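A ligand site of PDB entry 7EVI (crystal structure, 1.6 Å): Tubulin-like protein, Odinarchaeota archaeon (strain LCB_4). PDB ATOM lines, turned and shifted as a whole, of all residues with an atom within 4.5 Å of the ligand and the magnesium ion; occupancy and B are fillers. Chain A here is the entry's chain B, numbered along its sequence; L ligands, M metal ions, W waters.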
ATOM      1  N   VAL A  11     -10.761   8.449  15.474  1.00  0.00           N
ATOM      2  CA  VAL A  11     -11.096   7.662  16.661  1.00  0.00           C
ATOM      3  C   VAL A  11     -10.767   6.190  16.418  1.00  0.00           C
ATOM      4  O   VAL A  11     -11.311   5.587  15.475  1.00  0.00           O
ATOM      5  CB  VAL A  11     -12.575   7.810  17.026  1.00  0.00           C
ATOM      6  CG1 VAL A  11     -12.858   7.146  18.351  1.00  0.00           C
ATOM      7  CG2 VAL A  11     -13.012   9.327  17.053  1.00  0.00           C
ATOM      8  N   GLY A  12      -9.929   5.608  17.304  1.00  0.00           N
ATOM      9  CA  GLY A  12      -9.537   4.215  17.222  1.00  0.00           C
ATOM     10  C   GLY A  12      -8.483   3.960  16.162  1.00  0.00           C
ATOM     11  O   GLY A  12      -7.995   4.883  15.490  1.00  0.00           O
ATOM     12  N   GLN A  13      -8.099   2.676  16.015  1.00  0.00           N
ATOM     13  CA  GLN A  13      -6.975   2.354  15.128  1.00  0.00           C
ATOM     14  C   GLN A  13      -7.256   2.783  13.702  1.00  0.00           C
ATOM     15  O   GLN A  13      -6.468   3.507  13.061  1.00  0.00           O
ATOM     16  CB  GLN A  13      -6.636   0.851  15.192  1.00  0.00           C
ATOM     17  CG  GLN A  13      -5.489   0.470  14.187  1.00  0.00           C
ATOM     18  CD  GLN A  13      -4.653  -0.669  14.657  1.00  0.00           C
ATOM     19  OE1 GLN A  13      -5.119  -1.507  15.433  1.00  0.00           O
ATOM     20  NE2 GLN A  13      -3.404  -0.761  14.180  1.00  0.00           N
ATOM     21  N   GLY A  14      -8.377   2.329  13.160  1.00  0.00           N
ATOM     22  CA  GLY A  14      -8.691   2.662  11.787  1.00  0.00           C
ATOM     23  C   GLY A  14      -8.866   4.144  11.559  1.00  0.00           C
ATOM     24  O   GLY A  14      -8.348   4.693  10.580  1.00  0.00           O
ATOM     25  N   GLN A  17      -5.407   5.744  11.539  1.00  0.00           N
ATOM     26  CA  GLN A  17      -4.623   5.363  10.360  1.00  0.00           C
ATOM     27  C   GLN A  17      -5.161   6.057   9.098  1.00  0.00           C
ATOM     28  O   GLN A  17      -4.377   6.526   8.248  1.00  0.00           O
ATOM     29  CB  GLN A  17      -4.599   3.834  10.214  1.00  0.00           C
ATOM     30  CG  GLN A  17      -3.712   3.273  11.341  1.00  0.00           C
ATOM     31  CD  GLN A  17      -3.619   1.753  11.499  1.00  0.00           C
ATOM     32  OE1 GLN A  17      -2.768   1.301  12.259  1.00  0.00           O
ATOM     33  NE2 GLN A  17      -4.486   0.945  10.797  1.00  0.00           N
ATOM     34  N   ILE A  18      -6.476   6.163   8.984  1.00  0.00           N
ATOM     35  CA  ILE A  18      -7.080   6.867   7.842  1.00  0.00           C
ATOM     36  C   ILE A  18      -6.657   8.313   7.869  1.00  0.00           C
ATOM     37  O   ILE A  18      -6.374   8.929   6.831  1.00  0.00           O
ATOM     38  CB  ILE A  18      -8.605   6.728   7.885  1.00  0.00           C
ATOM     39  CG1 ILE A  18      -8.969   5.286   7.596  1.00  0.00           C
ATOM     40  CG2 ILE A  18      -9.248   7.716   6.893  1.00  0.00           C
ATOM     41  CD1 ILE A  18     -10.443   5.007   7.969  1.00  0.00           C
ATOM     42  N   ASP A  69      -7.745   7.745  20.953  1.00  0.00           N
ATOM     43  CA  ASP A  69      -7.846   6.275  21.019  1.00  0.00           C
ATOM     44  C   ASP A  69      -7.781   5.875  22.472  1.00  0.00           C
ATOM     45  O   ASP A  69      -7.227   6.608  23.311  1.00  0.00           O
ATOM     46  CB  ASP A  69      -6.710   5.622  20.219  1.00  0.00           C
ATOM     47  CG  ASP A  69      -7.035   4.209  19.755  1.00  0.00           C
ATOM     48  OD1 ASP A  69      -7.947   3.557  20.304  1.00  0.00           O
ATOM     49  OD2 ASP A  69      -6.377   3.756  18.790  1.00  0.00           O
ATOM     50  N   GLU A  71      -6.199   3.105  23.379  1.00  0.00           N
ATOM     51  CA  GLU A  71      -4.898   2.472  23.561  1.00  0.00           C
ATOM     52  C   GLU A  71      -3.923   3.276  22.732  1.00  0.00           C
ATOM     53  O   GLU A  71      -4.341   3.933  21.784  1.00  0.00           O
ATOM     54  CB  GLU A  71      -4.936   0.998  23.107  1.00  0.00           C
ATOM     55  CG  GLU A  71      -5.116   0.813  21.617  1.00  0.00           C
ATOM     56  CD  GLU A  71      -3.785   0.593  20.878  1.00  0.00           C
ATOM     57  OE1 GLU A  71      -3.774   0.770  19.637  1.00  0.00           O
ATOM     58  OE2 GLU A  71      -2.783   0.235  21.535  1.00  0.00           O
ATOM     59  N   GLY A  99      -7.693   0.104  26.211  1.00  0.00           N
ATOM     60  CA  GLY A  99      -8.378  -0.455  25.037  1.00  0.00           C
ATOM     61  C   GLY A  99      -9.863  -0.738  25.225  1.00  0.00           C
ATOM     62  O   GLY A  99     -10.302  -0.872  26.363  1.00  0.00           O
ATOM     63  N   ALA A 100     -10.658  -0.810  24.146  1.00  0.00           N
ATOM     64  CA  ALA A 100     -12.076  -1.147  24.284  1.00  0.00           C
ATOM     65  C   ALA A 100     -12.343  -2.624  24.045  1.00  0.00           C
ATOM     66  O   ALA A 100     -13.491  -3.072  24.207  1.00  0.00           O
ATOM     67  CB  ALA A 100     -12.954  -0.325  23.316  1.00  0.00           C
ATOM     68  N   HIS A 101     -11.307  -3.396  23.673  1.00  0.00           N
ATOM     69  CA  HIS A 101     -11.444  -4.864  23.541  1.00  0.00           C
ATOM     70  C   HIS A 101     -12.585  -5.246  22.607  1.00  0.00           C
ATOM     71  O   HIS A 101     -13.263  -6.265  22.825  1.00  0.00           O
ATOM     72  CB  HIS A 101     -11.624  -5.530  24.903  1.00  0.00           C
ATOM     73  CG  HIS A 101     -10.684  -5.035  25.953  1.00  0.00           C
ATOM     74  ND1 HIS A 101      -9.309  -5.006  25.804  1.00  0.00           N
ATOM     75  CD2 HIS A 101     -10.942  -4.558  27.194  1.00  0.00           C
ATOM     76  CE1 HIS A 101      -8.773  -4.493  26.905  1.00  0.00           C
ATOM     77  NE2 HIS A 101      -9.735  -4.228  27.763  1.00  0.00           N
ATOM     78  N   ASN A 102     -12.777  -4.439  21.542  1.00  0.00           N
ATOM     79  CA  ASN A 102     -13.757  -4.680  20.487  1.00  0.00           C
ATOM     80  C   ASN A 102     -15.213  -4.681  20.980  1.00  0.00           C
ATOM     81  O   ASN A 102     -16.085  -5.270  20.331  1.00  0.00           O
ATOM     82  CB  ASN A 102     -13.503  -6.011  19.783  1.00  0.00           C
ATOM     83  CG  ASN A 102     -12.386  -5.969  18.724  1.00  0.00           C
ATOM     84  OD1 ASN A 102     -12.150  -6.995  18.110  1.00  0.00           O
ATOM     85  ND2 ASN A 102     -11.690  -4.811  18.523  1.00  0.00           N
ATOM     86  N   THR A 138     -13.838   3.409  12.390  1.00  0.00           N
ATOM     87  CA  THR A 138     -14.436   2.154  11.950  1.00  0.00           C
ATOM     88  C   THR A 138     -15.601   1.789  12.883  1.00  0.00           C
ATOM     89  O   THR A 138     -15.656   2.217  14.040  1.00  0.00           O
ATOM     90  CB  THR A 138     -13.406   1.018  11.947  1.00  0.00           C
ATOM     91  OG1 THR A 138     -13.083   0.728  13.317  1.00  0.00           O
ATOM     92  CG2 THR A 138     -12.107   1.399  11.204  1.00  0.00           C
ATOM     93  N   GLY A 141     -14.843  -2.370  15.334  1.00  0.00           N
ATOM     94  CA  GLY A 141     -14.091  -2.446  16.570  1.00  0.00           C
ATOM     95  C   GLY A 141     -14.867  -1.846  17.735  1.00  0.00           C
ATOM     96  O   GLY A 141     -16.083  -1.688  17.681  1.00  0.00           O
ATOM     97  N   GLY A 142     -14.154  -1.537  18.834  1.00  0.00           N
ATOM     98  CA  GLY A 142     -14.828  -1.050  20.028  1.00  0.00           C
ATOM     99  C   GLY A 142     -14.674   0.446  20.299  1.00  0.00           C
ATOM    100  O   GLY A 142     -15.578   1.081  20.871  1.00  0.00           O
ATOM    101  N   THR A 143     -13.533   1.027  19.917  1.00  0.00           N
ATOM    102  CA  THR A 143     -13.260   2.436  20.225  1.00  0.00           C
ATOM    103  C   THR A 143     -13.824   3.346  19.139  1.00  0.00           C
ATOM    104  O   THR A 143     -14.631   4.236  19.422  1.00  0.00           O
ATOM    105  CB  THR A 143     -11.746   2.646  20.384  1.00  0.00           C
ATOM    106  OG1 THR A 143     -11.229   1.900  21.492  1.00  0.00           O
ATOM    107  CG2 THR A 143     -11.434   4.112  20.613  1.00  0.00           C
ATOM    108  N   GLY A 144     -13.385   3.135  17.885  1.00  0.00           N
ATOM    109  CA  GLY A 144     -14.046   3.825  16.782  1.00  0.00           C
ATOM    110  C   GLY A 144     -15.545   3.740  16.884  1.00  0.00           C
ATOM    111  O   GLY A 144     -16.253   4.733  16.736  1.00  0.00           O
ATOM    112  N   VAL A 169     -16.334   3.199   8.566  1.00  0.00           N
ATOM    113  CA  VAL A 169     -15.966   1.978   7.842  1.00  0.00           C
ATOM    114  C   VAL A 169     -16.813   0.818   8.356  1.00  0.00           C
ATOM    115  O   VAL A 169     -16.706   0.418   9.517  1.00  0.00           O
ATOM    116  CB  VAL A 169     -14.478   1.661   8.003  1.00  0.00           C
ATOM    117  CG1 VAL A 169     -14.099   0.484   7.071  1.00  0.00           C
ATOM    118  CG2 VAL A 169     -13.645   2.890   7.654  1.00  0.00           C
ATOM    119  N   ASP A 176     -14.017  -9.360  10.070  1.00  0.00           N
ATOM    120  CA  ASP A 176     -12.762  -9.721  10.729  1.00  0.00           C
ATOM    121  C   ASP A 176     -12.760  -9.366  12.212  1.00  0.00           C
ATOM    122  O   ASP A 176     -11.687  -9.319  12.848  1.00  0.00           O
ATOM    123  CB  ASP A 176     -11.573  -9.095  10.001  1.00  0.00           C
ATOM    124  CG  ASP A 176     -11.558  -7.624  10.073  1.00  0.00           C
ATOM    125  OD1 ASP A 176     -12.623  -7.005  10.154  1.00  0.00           O
ATOM    126  OD2 ASP A 176     -10.439  -7.065  10.014  1.00  0.00           O
ATOM    127  N   VAL A 177     -13.951  -9.141  12.763  1.00  0.00           N
ATOM    128  CA  VAL A 177     -14.222  -9.001  14.190  1.00  0.00           C
ATOM    129  C   VAL A 177     -15.547  -9.724  14.370  1.00  0.00           C
ATOM    130  O   VAL A 177     -16.552  -9.320  13.763  1.00  0.00           O
ATOM    131  CB  VAL A 177     -14.364  -7.523  14.629  1.00  0.00           C
ATOM    132  CG1 VAL A 177     -14.718  -7.422  16.118  1.00  0.00           C
ATOM    133  CG2 VAL A 177     -13.089  -6.734  14.298  1.00  0.00           C
ATOM    134  N   ASN A 203     -14.015  -2.515   3.620  1.00  0.00           N
ATOM    135  CA  ASN A 203     -12.733  -2.950   3.101  1.00  0.00           C
ATOM    136  C   ASN A 203     -12.852  -3.912   1.928  1.00  0.00           C
ATOM    137  O   ASN A 203     -11.925  -4.027   1.139  1.00  0.00           O
ATOM    138  CB  ASN A 203     -11.889  -3.570   4.212  1.00  0.00           C
ATOM    139  CG  ASN A 203     -11.431  -2.515   5.181  1.00  0.00           C
ATOM    140  OD1 ASN A 203     -11.449  -1.325   4.839  1.00  0.00           O
ATOM    141  ND2 ASN A 203     -11.013  -2.922   6.373  1.00  0.00           N
ATOM    142  N   LEU A 206     -13.008  -1.502  -0.905  1.00  0.00           N
ATOM    143  CA  LEU A 206     -11.733  -0.802  -1.063  1.00  0.00           C
ATOM    144  C   LEU A 206     -10.660  -1.719  -1.651  1.00  0.00           C
ATOM    145  O   LEU A 206      -9.898  -1.312  -2.555  1.00  0.00           O
ATOM    146  CB  LEU A 206     -11.270  -0.246   0.283  1.00  0.00           C
ATOM    147  CG  LEU A 206     -12.198   0.827   0.857  1.00  0.00           C
ATOM    148  CD1 LEU A 206     -11.702   1.278   2.255  1.00  0.00           C
ATOM    149  CD2 LEU A 206     -12.363   2.083  -0.078  1.00  0.00           C
ATOM    150  N   PHE A 222      -2.164  -0.544   5.642  1.00  0.00           N
ATOM    151  CA  PHE A 222      -3.461   0.071   5.374  1.00  0.00           C
ATOM    152  C   PHE A 222      -3.346   1.394   4.638  1.00  0.00           C
ATOM    153  O   PHE A 222      -4.365   1.869   4.123  1.00  0.00           O
ATOM    154  CB  PHE A 222      -4.280   0.289   6.647  1.00  0.00           C
ATOM    155  CG  PHE A 222      -5.199  -0.840   6.993  1.00  0.00           C
ATOM    156  CD1 PHE A 222      -6.183  -1.274   6.098  1.00  0.00           C
ATOM    157  CD2 PHE A 222      -5.115  -1.451   8.227  1.00  0.00           C
ATOM    158  CE1 PHE A 222      -7.047  -2.352   6.422  1.00  0.00           C
ATOM    159  CE2 PHE A 222      -5.986  -2.470   8.582  1.00  0.00           C
ATOM    160  CZ  PHE A 222      -6.947  -2.939   7.678  1.00  0.00           C
ATOM    161  N   ASN A 226      -6.338   3.074   2.659  1.00  0.00           N
ATOM    162  CA  ASN A 226      -6.985   4.250   3.235  1.00  0.00           C
ATOM    163  C   ASN A 226      -6.860   5.488   2.351  1.00  0.00           C
ATOM    164  O   ASN A 226      -7.604   6.451   2.560  1.00  0.00           O
ATOM    165  CB  ASN A 226      -6.355   4.574   4.600  1.00  0.00           C
ATOM    166  CG  ASN A 226      -6.648   3.561   5.624  1.00  0.00           C
ATOM    167  OD1 ASN A 226      -7.649   2.840   5.538  1.00  0.00           O
ATOM    168  ND2 ASN A 226      -5.813   3.506   6.662  1.00  0.00           N
ATOM    169  N   ILE A 229     -10.165   6.615   1.030  1.00  0.00           N
ATOM    170  CA  ILE A 229     -11.025   7.369   1.928  1.00  0.00           C
ATOM    171  C   ILE A 229     -10.562   8.810   2.012  1.00  0.00           C
ATOM    172  O   ILE A 229     -11.365   9.756   1.959  1.00  0.00           O
ATOM    173  CB  ILE A 229     -11.046   6.692   3.311  1.00  0.00           C
ATOM    174  CG1 ILE A 229     -11.525   5.243   3.150  1.00  0.00           C
ATOM    175  CG2 ILE A 229     -11.913   7.481   4.321  1.00  0.00           C
ATOM    176  CD1 ILE A 229     -11.460   4.477   4.496  1.00  0.00           C
HETATM  177  P1  LIG L   1     -10.603  -1.375  19.858  1.00  0.00           P
HETATM  178  O1  LIG L   1     -11.633  -2.417  20.050  1.00  0.00           O
HETATM  179  O2  LIG L   1      -9.287  -1.911  19.246  1.00  0.00           O
HETATM  180  O3  LIG L   1     -10.459  -0.523  21.082  1.00  0.00           O
HETATM  181  O4  LIG L   1     -11.320  -0.421  18.738  1.00  0.00           O
HETATM  182  P2  LIG L   1     -10.685   0.287  17.430  1.00  0.00           P
HETATM  183  O5  LIG L   1     -11.571   1.422  17.046  1.00  0.00           O
HETATM  184  O6  LIG L   1      -9.240   0.626  17.652  1.00  0.00           O
HETATM  185  O7  LIG L   1     -10.809  -0.915  16.389  1.00  0.00           O
HETATM  186  P3  LIG L   1     -10.281  -0.962  14.873  1.00  0.00           P
HETATM  187  O8  LIG L   1     -10.255   0.404  14.279  1.00  0.00           O
HETATM  188  O9  LIG L   1      -9.042  -1.841  14.804  1.00  0.00           O
HETATM  189  O10 LIG L   1     -11.525  -1.788  14.263  1.00  0.00           O
HETATM  190  C1  LIG L   1     -11.423  -3.031  13.625  1.00  0.00           C
HETATM  191  C2  LIG L   1     -12.103  -2.882  12.270  1.00  0.00           C
HETATM  192  O11 LIG L   1     -11.453  -1.808  11.569  1.00  0.00           O
HETATM  193  C3  LIG L   1     -11.845  -4.133  11.470  1.00  0.00           C
HETATM  194  O12 LIG L   1     -13.001  -4.337  10.651  1.00  0.00           O
HETATM  195  C4  LIG L   1     -10.568  -3.789  10.709  1.00  0.00           C
HETATM  196  O13 LIG L   1     -10.382  -4.464   9.501  1.00  0.00           O
HETATM  197  C5  LIG L   1     -10.772  -2.321  10.426  1.00  0.00           C
HETATM  198  N1  LIG L   1      -9.594  -1.470  10.345  1.00  0.00           N
HETATM  199  C6  LIG L   1      -8.664  -1.283  11.340  1.00  0.00           C
HETATM  200  N2  LIG L   1      -7.800  -0.349  10.925  1.00  0.00           N
HETATM  201  C7  LIG L   1      -8.149   0.044   9.664  1.00  0.00           C
HETATM  202  C8  LIG L   1      -7.630   0.984   8.770  1.00  0.00           C
HETATM  203  O14 LIG L   1      -6.626   1.671   8.957  1.00  0.00           O
HETATM  204  N3  LIG L   1      -8.277   1.150   7.568  1.00  0.00           N
HETATM  205  C9  LIG L   1      -9.416   0.436   7.232  1.00  0.00           C
HETATM  206  N4  LIG L   1     -10.009   0.629   6.030  1.00  0.00           N
HETATM  207  N5  LIG L   1      -9.938  -0.493   8.107  1.00  0.00           N
HETATM  208  C10 LIG L   1      -9.299  -0.647   9.313  1.00  0.00           C
HETATM  209 MG    MG M   1      -7.666  -0.498  18.672  1.00  0.00          MG
HETATM  210  O   HOH W   1     -15.118  -6.530   9.018  1.00  0.00           O
HETATM  211  O   HOH W   2     -12.622  -5.314   7.501  1.00  0.00           O
HETATM  212  O   HOH W   3      -9.334  -4.291  16.263  1.00  0.00           O
HETATM  213  O   HOH W   4     -13.589  -2.558   8.864  1.00  0.00           O
HETATM  214  O   HOH W   5      -7.353  -1.783  16.918  1.00  0.00           O
HETATM  215  O   HOH W   6     -11.487   3.238  14.230  1.00  0.00           O
HETATM  216  O   HOH W   7     -14.152   0.615  16.028  1.00  0.00           O
HETATM  217  O   HOH W   8      -6.225   0.972  18.419  1.00  0.00           O
HETATM  218  O   HOH W   9      -8.326   0.820  20.438  1.00  0.00           O
HETATM  219  O   HOH W  10     -15.436  -4.742  11.210  1.00  0.00           O
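The backbone NH (N) of Thr 143 lies within hydrogen-bond range of an oxygen (O4) of the ligand, at 2.9 Å.
An oxygen (O3) of the ligand is in hydrogen-bond range of the side-chain hydroxyl (OG1) of Thr 143 (2.6 Å).
O5 of the ligand sits at hydrogen-bond distance from N of Gly 144 (2.6 Å).
OD2 of Asp 176 sits at hydrogen-bond distance from O13 of the ligand (2.7 Å).
N4 of the ligand lies within hydrogen-bond range of OD1 of Asn 203, 2.7 Å away.
OD1 of Asn 226 is in hydrogen-bond range of N3 of the ligand (2.7 Å).
N of Asn 102 is in hydrogen-bond range of O1 of the ligand, at 2.8 Å.
The side-chain amide nitrogen (ND2) of Asn 102 sits at hydrogen-bond distance from an oxygen (O1) of the ligand, at 2.8 Å.
O6 of the ligand sits close to N of Gln 13 (2.9 Å).
An oxygen (O8) of the ligand is in hydrogen-bond range of the backbone NH (N) of Gly 14, 2.9 Å away.
O14 of the ligand lies within hydrogen-bond range of NE2 of Gln 17.
An oxygen (O1) of the ligand is in hydrogen-bond range of the backbone NH (N) of Gly 142 (2.9 Å).
The side-chain hydroxyl (OG1) of Thr 138 sits at hydrogen-bond distance from an oxygen (O8) of the ligand, at 3.0 Å.
The backbone NH (N) of Ala 100 is in hydrogen-bond range of an oxygen (O3) of the ligand.
The backbone carbonyl oxygen of Phe 222 lies close to the side-chain amide nitrogen of Asn 226 (3.4 Å).
NE2 of Gln 13 is in hydrogen-bond range of OE1 of Gln 17 (2.9 Å).
The side-chain carboxylate (OD2) of Asp 69 is in hydrogen-bond range of the backbone NH (N) of Gln 13, at 3.4 Å.
The magnesium ion is bound by water W8 (2.1 Å), O6 of the ligand (2.2 Å), water W5 (2.2 Å), O2 of the ligand (2.2 Å) and water W9 (2.3 Å).
The magnesium ion has five donor atoms within binding distance.
Water W8 lies within hydrogen-bond range of the side-chain carboxylate of Glu 71, the side-chain carboxylate of Asp 69 and the backbone NH of Gln 13.
Water W5 lies within hydrogen-bond range of the side-chain amide oxygen of Gln 13 and an oxygen (O9) of the ligand.
Water W3 lies within hydrogen-bond range of O9 of the ligand and ND2 of Asn 102.
Water W7 lies within hydrogen-bond range of O5 of the ligand (2.9 Å), OG1 of Thr 138 (2.9 Å), N of Gly 141 (3.1 Å) and N of Gly 144 (3.2 Å).
Water W6 lies within hydrogen-bond range of the backbone carbonyl oxygen of Val 11, the backbone NH of Thr 138, an oxygen (O8) of the ligand and the backbone NH of Gly 14.
Water W2 lies within hydrogen-bond range of ND2 of Asn 203, O13 of the ligand and OD1 of Asp 176.
CB of Gln 13 touches the magnesium ion, 3.9 Å away.
The nearest printed residue that does not touch the magnesium ion is Glu 71 (4.1 Å).
Merely in contact with the ligand: Gly 12 (3.5 Å), Phe 222 (3.5 Å), Gly 141 (3.5 Å) and His 101 (3.8 Å).
Hydrophobic or aromatic side chains within 4 Å of the ligand: Ala 100 and Phe 222.
The nearest printed residue that does not touch the ligand is Val 177 (4.04 Å).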
